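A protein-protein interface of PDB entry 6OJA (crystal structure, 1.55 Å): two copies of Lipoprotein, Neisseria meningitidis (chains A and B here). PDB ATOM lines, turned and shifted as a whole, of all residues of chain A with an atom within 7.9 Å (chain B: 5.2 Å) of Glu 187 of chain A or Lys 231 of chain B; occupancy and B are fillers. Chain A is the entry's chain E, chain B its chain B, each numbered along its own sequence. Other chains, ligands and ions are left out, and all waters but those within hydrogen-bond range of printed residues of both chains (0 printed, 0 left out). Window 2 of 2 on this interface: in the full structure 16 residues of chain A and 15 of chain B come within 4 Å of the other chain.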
ATOM      1  N   GLY A  88      16.128  18.698  -3.480  1.00  0.00           N
ATOM      2  CA  GLY A  88      16.066  18.846  -4.923  1.00  0.00           C
ATOM      3  C   GLY A  88      17.191  18.115  -5.623  1.00  0.00           C
ATOM      4  O   GLY A  88      18.293  17.976  -5.102  1.00  0.00           O
ATOM      5  N   LEU A  89      16.900  17.677  -6.861  1.00  0.00           N
ATOM      6  CA  LEU A  89      17.926  17.255  -7.808  1.00  0.00           C
ATOM      7  C   LEU A  89      18.206  18.441  -8.716  1.00  0.00           C
ATOM      8  O   LEU A  89      17.275  18.991  -9.306  1.00  0.00           O
ATOM      9  CB  LEU A  89      17.463  16.038  -8.620  1.00  0.00           C
ATOM     10  CG  LEU A  89      18.504  15.422  -9.543  1.00  0.00           C
ATOM     11  CD1 LEU A  89      18.259  13.931  -9.699  1.00  0.00           C
ATOM     12  CD2 LEU A  89      18.457  16.104 -10.912  1.00  0.00           C
ATOM     13  N   TYR A  90      19.466  18.849  -8.788  1.00  0.00           N
ATOM     14  CA  TYR A  90      19.877  20.074  -9.442  1.00  0.00           C
ATOM     15  C   TYR A  90      20.812  19.759 -10.593  1.00  0.00           C
ATOM     16  O   TYR A  90      21.483  18.721 -10.603  1.00  0.00           O
ATOM     17  CB  TYR A  90      20.604  21.003  -8.454  1.00  0.00           C
ATOM     18  CG  TYR A  90      19.716  21.541  -7.371  1.00  0.00           C
ATOM     19  CD1 TYR A  90      19.547  20.850  -6.172  1.00  0.00           C
ATOM     20  CD2 TYR A  90      19.106  22.766  -7.507  1.00  0.00           C
ATOM     21  CE1 TYR A  90      18.726  21.347  -5.177  1.00  0.00           C
ATOM     22  CE2 TYR A  90      18.294  23.283  -6.528  1.00  0.00           C
ATOM     23  CZ  TYR A  90      18.125  22.577  -5.345  1.00  0.00           C
ATOM     24  OH  TYR A  90      17.319  23.115  -4.369  1.00  0.00           O
ATOM     25  N   PRO A  91      20.907  20.652 -11.566  1.00  0.00           N
ATOM     26  CA  PRO A  91      21.869  20.438 -12.641  1.00  0.00           C
ATOM     27  C   PRO A  91      23.297  20.486 -12.128  1.00  0.00           C
ATOM     28  O   PRO A  91      23.662  21.339 -11.316  1.00  0.00           O
ATOM     29  CB  PRO A  91      21.577  21.581 -13.624  1.00  0.00           C
ATOM     30  CG  PRO A  91      20.713  22.547 -12.914  1.00  0.00           C
ATOM     31  CD  PRO A  91      20.081  21.851 -11.737  1.00  0.00           C
ATOM     32  N   LYS A  95      22.214  19.637 -17.698  1.00  0.00           N
ATOM     33  CA  LYS A  95      21.361  20.772 -17.373  1.00  0.00           C
ATOM     34  C   LYS A  95      19.871  20.466 -17.394  1.00  0.00           C
ATOM     35  O   LYS A  95      19.073  21.340 -17.039  1.00  0.00           O
ATOM     36  CB  LYS A  95      21.641  21.935 -18.335  1.00  0.00           C
ATOM     37  CG  LYS A  95      23.110  22.333 -18.386  1.00  0.00           C
ATOM     38  CD  LYS A  95      23.695  22.584 -16.999  1.00  0.00           C
ATOM     39  CE  LYS A  95      25.147  23.046 -17.089  1.00  0.00           C
ATOM     40  NZ  LYS A  95      25.705  23.319 -15.743  1.00  0.00           N
ATOM     41  N   ARG A 165      28.582  19.724  -8.007  1.00  0.00           N
ATOM     42  CA  ARG A 165      27.978  19.977  -9.310  1.00  0.00           C
ATOM     43  C   ARG A 165      29.025  20.152 -10.398  1.00  0.00           C
ATOM     44  O   ARG A 165      28.704  19.999 -11.585  1.00  0.00           O
ATOM     45  CB  ARG A 165      27.092  21.209  -9.244  1.00  0.00           C
ATOM     46  CG  ARG A 165      25.818  20.993  -8.467  1.00  0.00           C
ATOM     47  CD  ARG A 165      25.056  22.269  -8.367  1.00  0.00           C
ATOM     48  NE  ARG A 165      25.803  23.232  -7.572  1.00  0.00           N
ATOM     49  CZ  ARG A 165      25.561  24.535  -7.551  1.00  0.00           C
ATOM     50  NH1 ARG A 165      24.581  25.048  -8.293  1.00  0.00           N
ATOM     51  NH2 ARG A 165      26.309  25.328  -6.792  1.00  0.00           N
ATOM     52  N   ILE A 179      20.397  26.488  -0.172  1.00  0.00           N
ATOM     53  CA  ILE A 179      20.192  27.909   0.125  1.00  0.00           C
ATOM     54  C   ILE A 179      21.509  28.580   0.486  1.00  0.00           C
ATOM     55  O   ILE A 179      21.849  29.644  -0.052  1.00  0.00           O
ATOM     56  CB  ILE A 179      19.153  28.080   1.248  1.00  0.00           C
ATOM     57  CG1 ILE A 179      17.776  27.615   0.772  1.00  0.00           C
ATOM     58  CG2 ILE A 179      19.131  29.543   1.751  1.00  0.00           C
ATOM     59  CD1 ILE A 179      17.252  28.326  -0.481  1.00  0.00           C
ATOM     60  N   SER A 181      24.525  27.892  -0.145  1.00  0.00           N
ATOM     61  CA  SER A 181      25.571  27.941  -1.155  1.00  0.00           C
ATOM     62  C   SER A 181      25.188  28.862  -2.297  1.00  0.00           C
ATOM     63  O   SER A 181      25.922  28.951  -3.290  1.00  0.00           O
ATOM     64  CB  SER A 181      25.885  26.535  -1.667  1.00  0.00           C
ATOM     65  OG  SER A 181      24.793  26.031  -2.400  1.00  0.00           O
ATOM     66  N   GLY A 182      24.057  29.548  -2.183  1.00  0.00           N
ATOM     67  CA  GLY A 182      23.633  30.446  -3.240  1.00  0.00           C
ATOM     68  C   GLY A 182      22.902  29.761  -4.366  1.00  0.00           C
ATOM     69  O   GLY A 182      22.857  30.288  -5.484  1.00  0.00           O
ATOM     70  N   MET A 183      22.346  28.582  -4.122  1.00  0.00           N
ATOM     71  CA  MET A 183      21.483  27.920  -5.078  1.00  0.00           C
ATOM     72  C   MET A 183      20.051  28.360  -4.851  1.00  0.00           C
ATOM     73  O   MET A 183      19.687  28.828  -3.775  1.00  0.00           O
ATOM     74  CB  MET A 183      21.598  26.395  -4.938  1.00  0.00           C
ATOM     75  CG  MET A 183      22.966  25.857  -5.278  1.00  0.00           C
ATOM     76  SD  MET A 183      23.234  24.120  -4.816  1.00  0.00           S
ATOM     77  CE  MET A 183      22.122  23.283  -5.951  1.00  0.00           C
ATOM     78  N   LYS A 184      19.229  28.248  -5.895  1.00  0.00           N
ATOM     79  CA  LYS A 184      17.821  28.584  -5.777  1.00  0.00           C
ATOM     80  C   LYS A 184      16.979  27.332  -5.910  1.00  0.00           C
ATOM     81  O   LYS A 184      17.200  26.503  -6.803  1.00  0.00           O
ATOM     82  CB  LYS A 184      17.390  29.612  -6.831  1.00  0.00           C
ATOM     83  CG  LYS A 184      18.184  30.896  -6.814  1.00  0.00           C
ATOM     84  CD  LYS A 184      18.095  31.547  -5.466  1.00  0.00           C
ATOM     85  CE  LYS A 184      17.758  33.012  -5.568  1.00  0.00           C
ATOM     86  NZ  LYS A 184      18.149  33.684  -4.308  1.00  0.00           N
ATOM     87  N   LEU A 185      15.973  27.227  -5.050  1.00  0.00           N
ATOM     88  CA  LEU A 185      15.130  26.036  -5.054  1.00  0.00           C
ATOM     89  C   LEU A 185      14.394  25.881  -6.373  1.00  0.00           C
ATOM     90  O   LEU A 185      14.191  24.756  -6.845  1.00  0.00           O
ATOM     91  CB  LEU A 185      14.147  26.107  -3.892  1.00  0.00           C
ATOM     92  CG  LEU A 185      14.837  26.206  -2.521  1.00  0.00           C
ATOM     93  CD1 LEU A 185      13.843  26.621  -1.453  1.00  0.00           C
ATOM     94  CD2 LEU A 185      15.532  24.904  -2.101  1.00  0.00           C
ATOM     95  N   THR A 186      13.989  26.995  -6.978  1.00  0.00           N
ATOM     96  CA  THR A 186      13.287  26.962  -8.255  1.00  0.00           C
ATOM     97  C   THR A 186      14.153  26.489  -9.410  1.00  0.00           C
ATOM     98  O   THR A 186      13.608  26.222 -10.488  1.00  0.00           O
ATOM     99  CB  THR A 186      12.735  28.348  -8.580  1.00  0.00           C
ATOM    100  OG1 THR A 186      13.804  29.295  -8.559  1.00  0.00           O
ATOM    101  CG2 THR A 186      11.699  28.738  -7.552  1.00  0.00           C
ATOM    102  N   GLU A 187      15.467  26.393  -9.238  1.00  0.00           N
ATOM    103  CA  GLU A 187      16.326  25.865 -10.291  1.00  0.00           C
ATOM    104  C   GLU A 187      16.526  24.362 -10.194  1.00  0.00           C
ATOM    105  O   GLU A 187      17.217  23.789 -11.042  1.00  0.00           O
ATOM    106  CB  GLU A 187      17.682  26.572 -10.282  1.00  0.00           C
ATOM    107  CG  GLU A 187      17.499  28.065 -10.197  1.00  0.00           C
ATOM    108  CD  GLU A 187      18.741  28.873 -10.539  1.00  0.00           C
ATOM    109  OE1 GLU A 187      18.583  30.012 -11.054  1.00  0.00           O
ATOM    110  OE2 GLU A 187      19.863  28.379 -10.295  1.00  0.00           O
ATOM    111  N   ALA A 188      15.951  23.712  -9.184  1.00  0.00           N
ATOM    112  CA  ALA A 188      15.961  22.260  -9.146  1.00  0.00           C
ATOM    113  C   ALA A 188      15.218  21.704 -10.346  1.00  0.00           C
ATOM    114  O   ALA A 188      14.173  22.232 -10.750  1.00  0.00           O
ATOM    115  CB  ALA A 188      15.308  21.742  -7.868  1.00  0.00           C
ATOM    116  N   LEU A 189      15.761  20.623 -10.900  1.00  0.00           N
ATOM    117  CA  LEU A 189      15.088  19.863 -11.955  1.00  0.00           C
ATOM    118  C   LEU A 189      13.962  19.000 -11.409  1.00  0.00           C
ATOM    119  O   LEU A 189      13.035  18.655 -12.149  1.00  0.00           O
ATOM    120  CB  LEU A 189      16.104  18.977 -12.683  1.00  0.00           C
ATOM    121  CG  LEU A 189      17.342  19.658 -13.274  1.00  0.00           C
ATOM    122  CD1 LEU A 189      18.233  18.660 -14.013  1.00  0.00           C
ATOM    123  CD2 LEU A 189      16.972  20.839 -14.176  1.00  0.00           C
ATOM    124  N   PHE A 190      14.021  18.657 -10.125  1.00  0.00           N
ATOM    125  CA  PHE A 190      13.019  17.810  -9.503  1.00  0.00           C
ATOM    126  C   PHE A 190      13.086  18.069  -8.009  1.00  0.00           C
ATOM    127  O   PHE A 190      14.181  18.097  -7.447  1.00  0.00           O
ATOM    128  CB  PHE A 190      13.251  16.330  -9.786  1.00  0.00           C
ATOM    129  CG  PHE A 190      12.178  15.428  -9.232  1.00  0.00           C
ATOM    130  CD1 PHE A 190      11.048  15.133  -9.979  1.00  0.00           C
ATOM    131  CD2 PHE A 190      12.302  14.860  -7.978  1.00  0.00           C
ATOM    132  CE1 PHE A 190      10.061  14.300  -9.472  1.00  0.00           C
ATOM    133  CE2 PHE A 190      11.309  14.016  -7.469  1.00  0.00           C
ATOM    134  CZ  PHE A 190      10.193  13.739  -8.231  1.00  0.00           C
ATOM    135  N   GLN A 191      11.933  18.287  -7.393  1.00  0.00           N
ATOM    136  CA  GLN A 191      11.828  18.507  -5.957  1.00  0.00           C
ATOM    137  C   GLN A 191      11.078  17.342  -5.322  1.00  0.00           C
ATOM    138  O   GLN A 191      10.039  16.906  -5.833  1.00  0.00           O
ATOM    139  CB  GLN A 191      11.111  19.830  -5.687  1.00  0.00           C
ATOM    140  CG  GLN A 191      10.989  20.264  -4.264  1.00  0.00           C
ATOM    141  CD  GLN A 191      10.427  21.674  -4.190  1.00  0.00           C
ATOM    142  OE1 GLN A 191       9.348  21.898  -3.638  1.00  0.00           O
ATOM    143  NE2 GLN A 191      11.145  22.620  -4.784  1.00  0.00           N
ATOM    144  N   ALA B 227      30.316  34.419  -7.040  1.00  0.00           N
ATOM    145  CA  ALA B 227      29.347  33.444  -7.526  1.00  0.00           C
ATOM    146  C   ALA B 227      28.239  33.217  -6.503  1.00  0.00           C
ATOM    147  O   ALA B 227      27.051  33.207  -6.846  1.00  0.00           O
ATOM    148  CB  ALA B 227      30.068  32.132  -7.849  1.00  0.00           C
ATOM    149  N   TYR B 228      28.618  33.052  -5.231  1.00  0.00           N
ATOM    150  CA  TYR B 228      27.638  32.860  -4.167  1.00  0.00           C
ATOM    151  C   TYR B 228      26.723  34.066  -4.055  1.00  0.00           C
ATOM    152  O   TYR B 228      25.500  33.928  -3.959  1.00  0.00           O
ATOM    153  CB  TYR B 228      28.376  32.588  -2.843  1.00  0.00           C
ATOM    154  CG  TYR B 228      27.684  33.011  -1.558  1.00  0.00           C
ATOM    155  CD1 TYR B 228      26.792  32.177  -0.897  1.00  0.00           C
ATOM    156  CD2 TYR B 228      27.987  34.221  -0.954  1.00  0.00           C
ATOM    157  CE1 TYR B 228      26.190  32.555   0.292  1.00  0.00           C
ATOM    158  CE2 TYR B 228      27.387  34.607   0.227  1.00  0.00           C
ATOM    159  CZ  TYR B 228      26.507  33.788   0.859  1.00  0.00           C
ATOM    160  OH  TYR B 228      25.923  34.184   2.031  1.00  0.00           O
ATOM    161  N   ALA B 229      27.305  35.263  -4.034  1.00  0.00           N
ATOM    162  CA  ALA B 229      26.514  36.463  -3.793  1.00  0.00           C
ATOM    163  C   ALA B 229      25.526  36.728  -4.921  1.00  0.00           C
ATOM    164  O   ALA B 229      24.412  37.199  -4.676  1.00  0.00           O
ATOM    165  CB  ALA B 229      27.433  37.665  -3.614  1.00  0.00           C
ATOM    166  N   HIS B 230      25.918  36.444  -6.167  1.00  0.00           N
ATOM    167  CA  HIS B 230      25.066  36.820  -7.294  1.00  0.00           C
ATOM    168  C   HIS B 230      23.698  36.143  -7.225  1.00  0.00           C
ATOM    169  O   HIS B 230      22.705  36.710  -7.685  1.00  0.00           O
ATOM    170  CB  HIS B 230      25.779  36.511  -8.616  1.00  0.00           C
ATOM    171  CG  HIS B 230      26.833  37.518  -8.987  1.00  0.00           C
ATOM    172  ND1 HIS B 230      28.027  37.166  -9.585  1.00  0.00           N
ATOM    173  CD2 HIS B 230      26.869  38.868  -8.852  1.00  0.00           C
ATOM    174  CE1 HIS B 230      28.754  38.250  -9.794  1.00  0.00           C
ATOM    175  NE2 HIS B 230      28.075  39.297  -9.358  1.00  0.00           N
ATOM    176  N   LYS B 231      23.603  34.970  -6.606  1.00  0.00           N
ATOM    177  CA  LYS B 231      22.317  34.297  -6.481  1.00  0.00           C
ATOM    178  C   LYS B 231      21.750  34.287  -5.074  1.00  0.00           C
ATOM    179  O   LYS B 231      20.530  34.293  -4.913  1.00  0.00           O
ATOM    180  CB  LYS B 231      22.453  32.869  -7.005  1.00  0.00           C
ATOM    181  CG  LYS B 231      22.791  32.886  -8.487  1.00  0.00           C
ATOM    182  CD  LYS B 231      21.575  32.601  -9.309  1.00  0.00           C
ATOM    183  CE  LYS B 231      21.218  31.146  -9.211  1.00  0.00           C
ATOM    184  NZ  LYS B 231      21.253  30.528 -10.564  1.00  0.00           N
ATOM    185  N   ARG B 232      22.588  34.301  -4.039  1.00  0.00           N
ATOM    186  CA  ARG B 232      22.049  34.428  -2.693  1.00  0.00           C
ATOM    187  C   ARG B 232      21.374  35.778  -2.504  1.00  0.00           C
ATOM    188  O   ARG B 232      20.338  35.870  -1.829  1.00  0.00           O
ATOM    189  CB  ARG B 232      23.161  34.254  -1.667  1.00  0.00           C
ATOM    190  CG  ARG B 232      22.686  34.217  -0.218  1.00  0.00           C
ATOM    191  CD  ARG B 232      22.044  32.889   0.131  1.00  0.00           C
ATOM    192  NE  ARG B 232      21.924  32.673   1.569  1.00  0.00           N
ATOM    193  CZ  ARG B 232      20.806  32.757   2.289  1.00  0.00           C
ATOM    194  NH1 ARG B 232      19.644  33.083   1.735  1.00  0.00           N
ATOM    195  NH2 ARG B 232      20.846  32.486   3.584  1.00  0.00           N
ATOM    196  N   PHE B 233      21.947  36.825  -3.092  1.00  0.00           N
ATOM    197  CA  PHE B 233      21.508  38.210  -2.888  1.00  0.00           C
ATOM    198  C   PHE B 233      21.120  38.828  -4.229  1.00  0.00           C
ATOM    199  O   PHE B 233      21.762  39.749  -4.746  1.00  0.00           O
ATOM    200  CB  PHE B 233      22.606  38.986  -2.184  1.00  0.00           C
ATOM    201  CG  PHE B 233      23.070  38.323  -0.907  1.00  0.00           C
ATOM    202  CD1 PHE B 233      22.230  38.223   0.180  1.00  0.00           C
ATOM    203  CD2 PHE B 233      24.332  37.776  -0.819  1.00  0.00           C
ATOM    204  CE1 PHE B 233      22.640  37.601   1.332  1.00  0.00           C
ATOM    205  CE2 PHE B 233      24.741  37.158   0.325  1.00  0.00           C
ATOM    206  CZ  PHE B 233      23.898  37.068   1.399  1.00  0.00           C
ATOM    207  N   GLU B 234      20.054  38.297  -4.808  1.00  0.00           N
ATOM    208  CA  GLU B 234      19.588  38.813  -6.080  1.00  0.00           C
ATOM    209  C   GLU B 234      19.035  40.214  -5.903  1.00  0.00           C
ATOM    210  O   GLU B 234      18.345  40.519  -4.926  1.00  0.00           O
ATOM    211  CB  GLU B 234      18.530  37.882  -6.672  1.00  0.00           C
ATOM    212  CG  GLU B 234      19.124  36.557  -7.118  1.00  0.00           C
ATOM    213  CD  GLU B 234      18.181  35.722  -7.959  1.00  0.00           C
ATOM    214  OE1 GLU B 234      16.954  35.751  -7.708  1.00  0.00           O
ATOM    215  OE2 GLU B 234      18.682  35.038  -8.876  1.00  0.00           O
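The side-chain carboxylate (OE2) of Glu 187 of chain A lies within salt-bridge range of the side-chain amino group (NZ) of Lys 231 of chain B (2.6 Å). The backbone carbonyl oxygen (O) of Lys 231 of chain B lies within hydrogen-bond range of the side-chain amino group (NZ) of Lys 184 of chain A (2.5 Å). The backbone carbonyl oxygen (O) of Ile 179 of chain A lies close to the guanidinium group (NE) of Arg 232 of chain B, at 3.4 Å.
Of the 8 printed residues of chain B, 4 touch a printed residue of chain A. Hydrophobic or aromatic side chains of chain B that line the printed part of chain A: Tyr 228. Hydrophobic or aromatic side chains of chain A within 4 Å of the printed part of chain B: Ile 179.
The side-chain sulfur of Met 183 of chain A lies close to the side-chain hydroxyl of Ser 181 of chain A (3.5 Å).
C of Ser 181 of chain A touches CD1 of Tyr 228 of chain B, 3.9 Å away. Gly 182 of chain A touches Lys 231 of chain B (O to CB, 3.0 Å). NZ of Lys 184 of chain A touches O of Arg 232 of chain B (3.96 Å). Lys 184 of chain A touches Glu 234 of chain B (CE to OE1, 3.6 Å).
No position is printed for both chains. Of the 7 pairs that touch across the chains among the printed residues, none has its exchanged pair printed and touching as well.
Arg 165 of chain A touches none of the printed residues of chain B. Printed residues of chain B within 4 Å of Ile 179 of chain A: Arg 232. Of the printed residues of chain B, Ser 181 of chain A touches Tyr 228 (3.9 Å). Printed residues of chain B within 4 Å of Gly 182 of chain A: Lys 231. Glu 187 of chain A touches one residue of chain B. Of the printed residues of chain A, Lys 231 of chain B touches Gly 182 (3.0 Å), Lys 184 (2.5 Å) and Glu 187 (2.6 Å). Of the printed residues of chain A, Glu 234 of chain B touches Lys 184. The nearest printed residue of chain A that does not touch Arg 232 of chain B is Gly 182 of chain A (4.1 Å).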
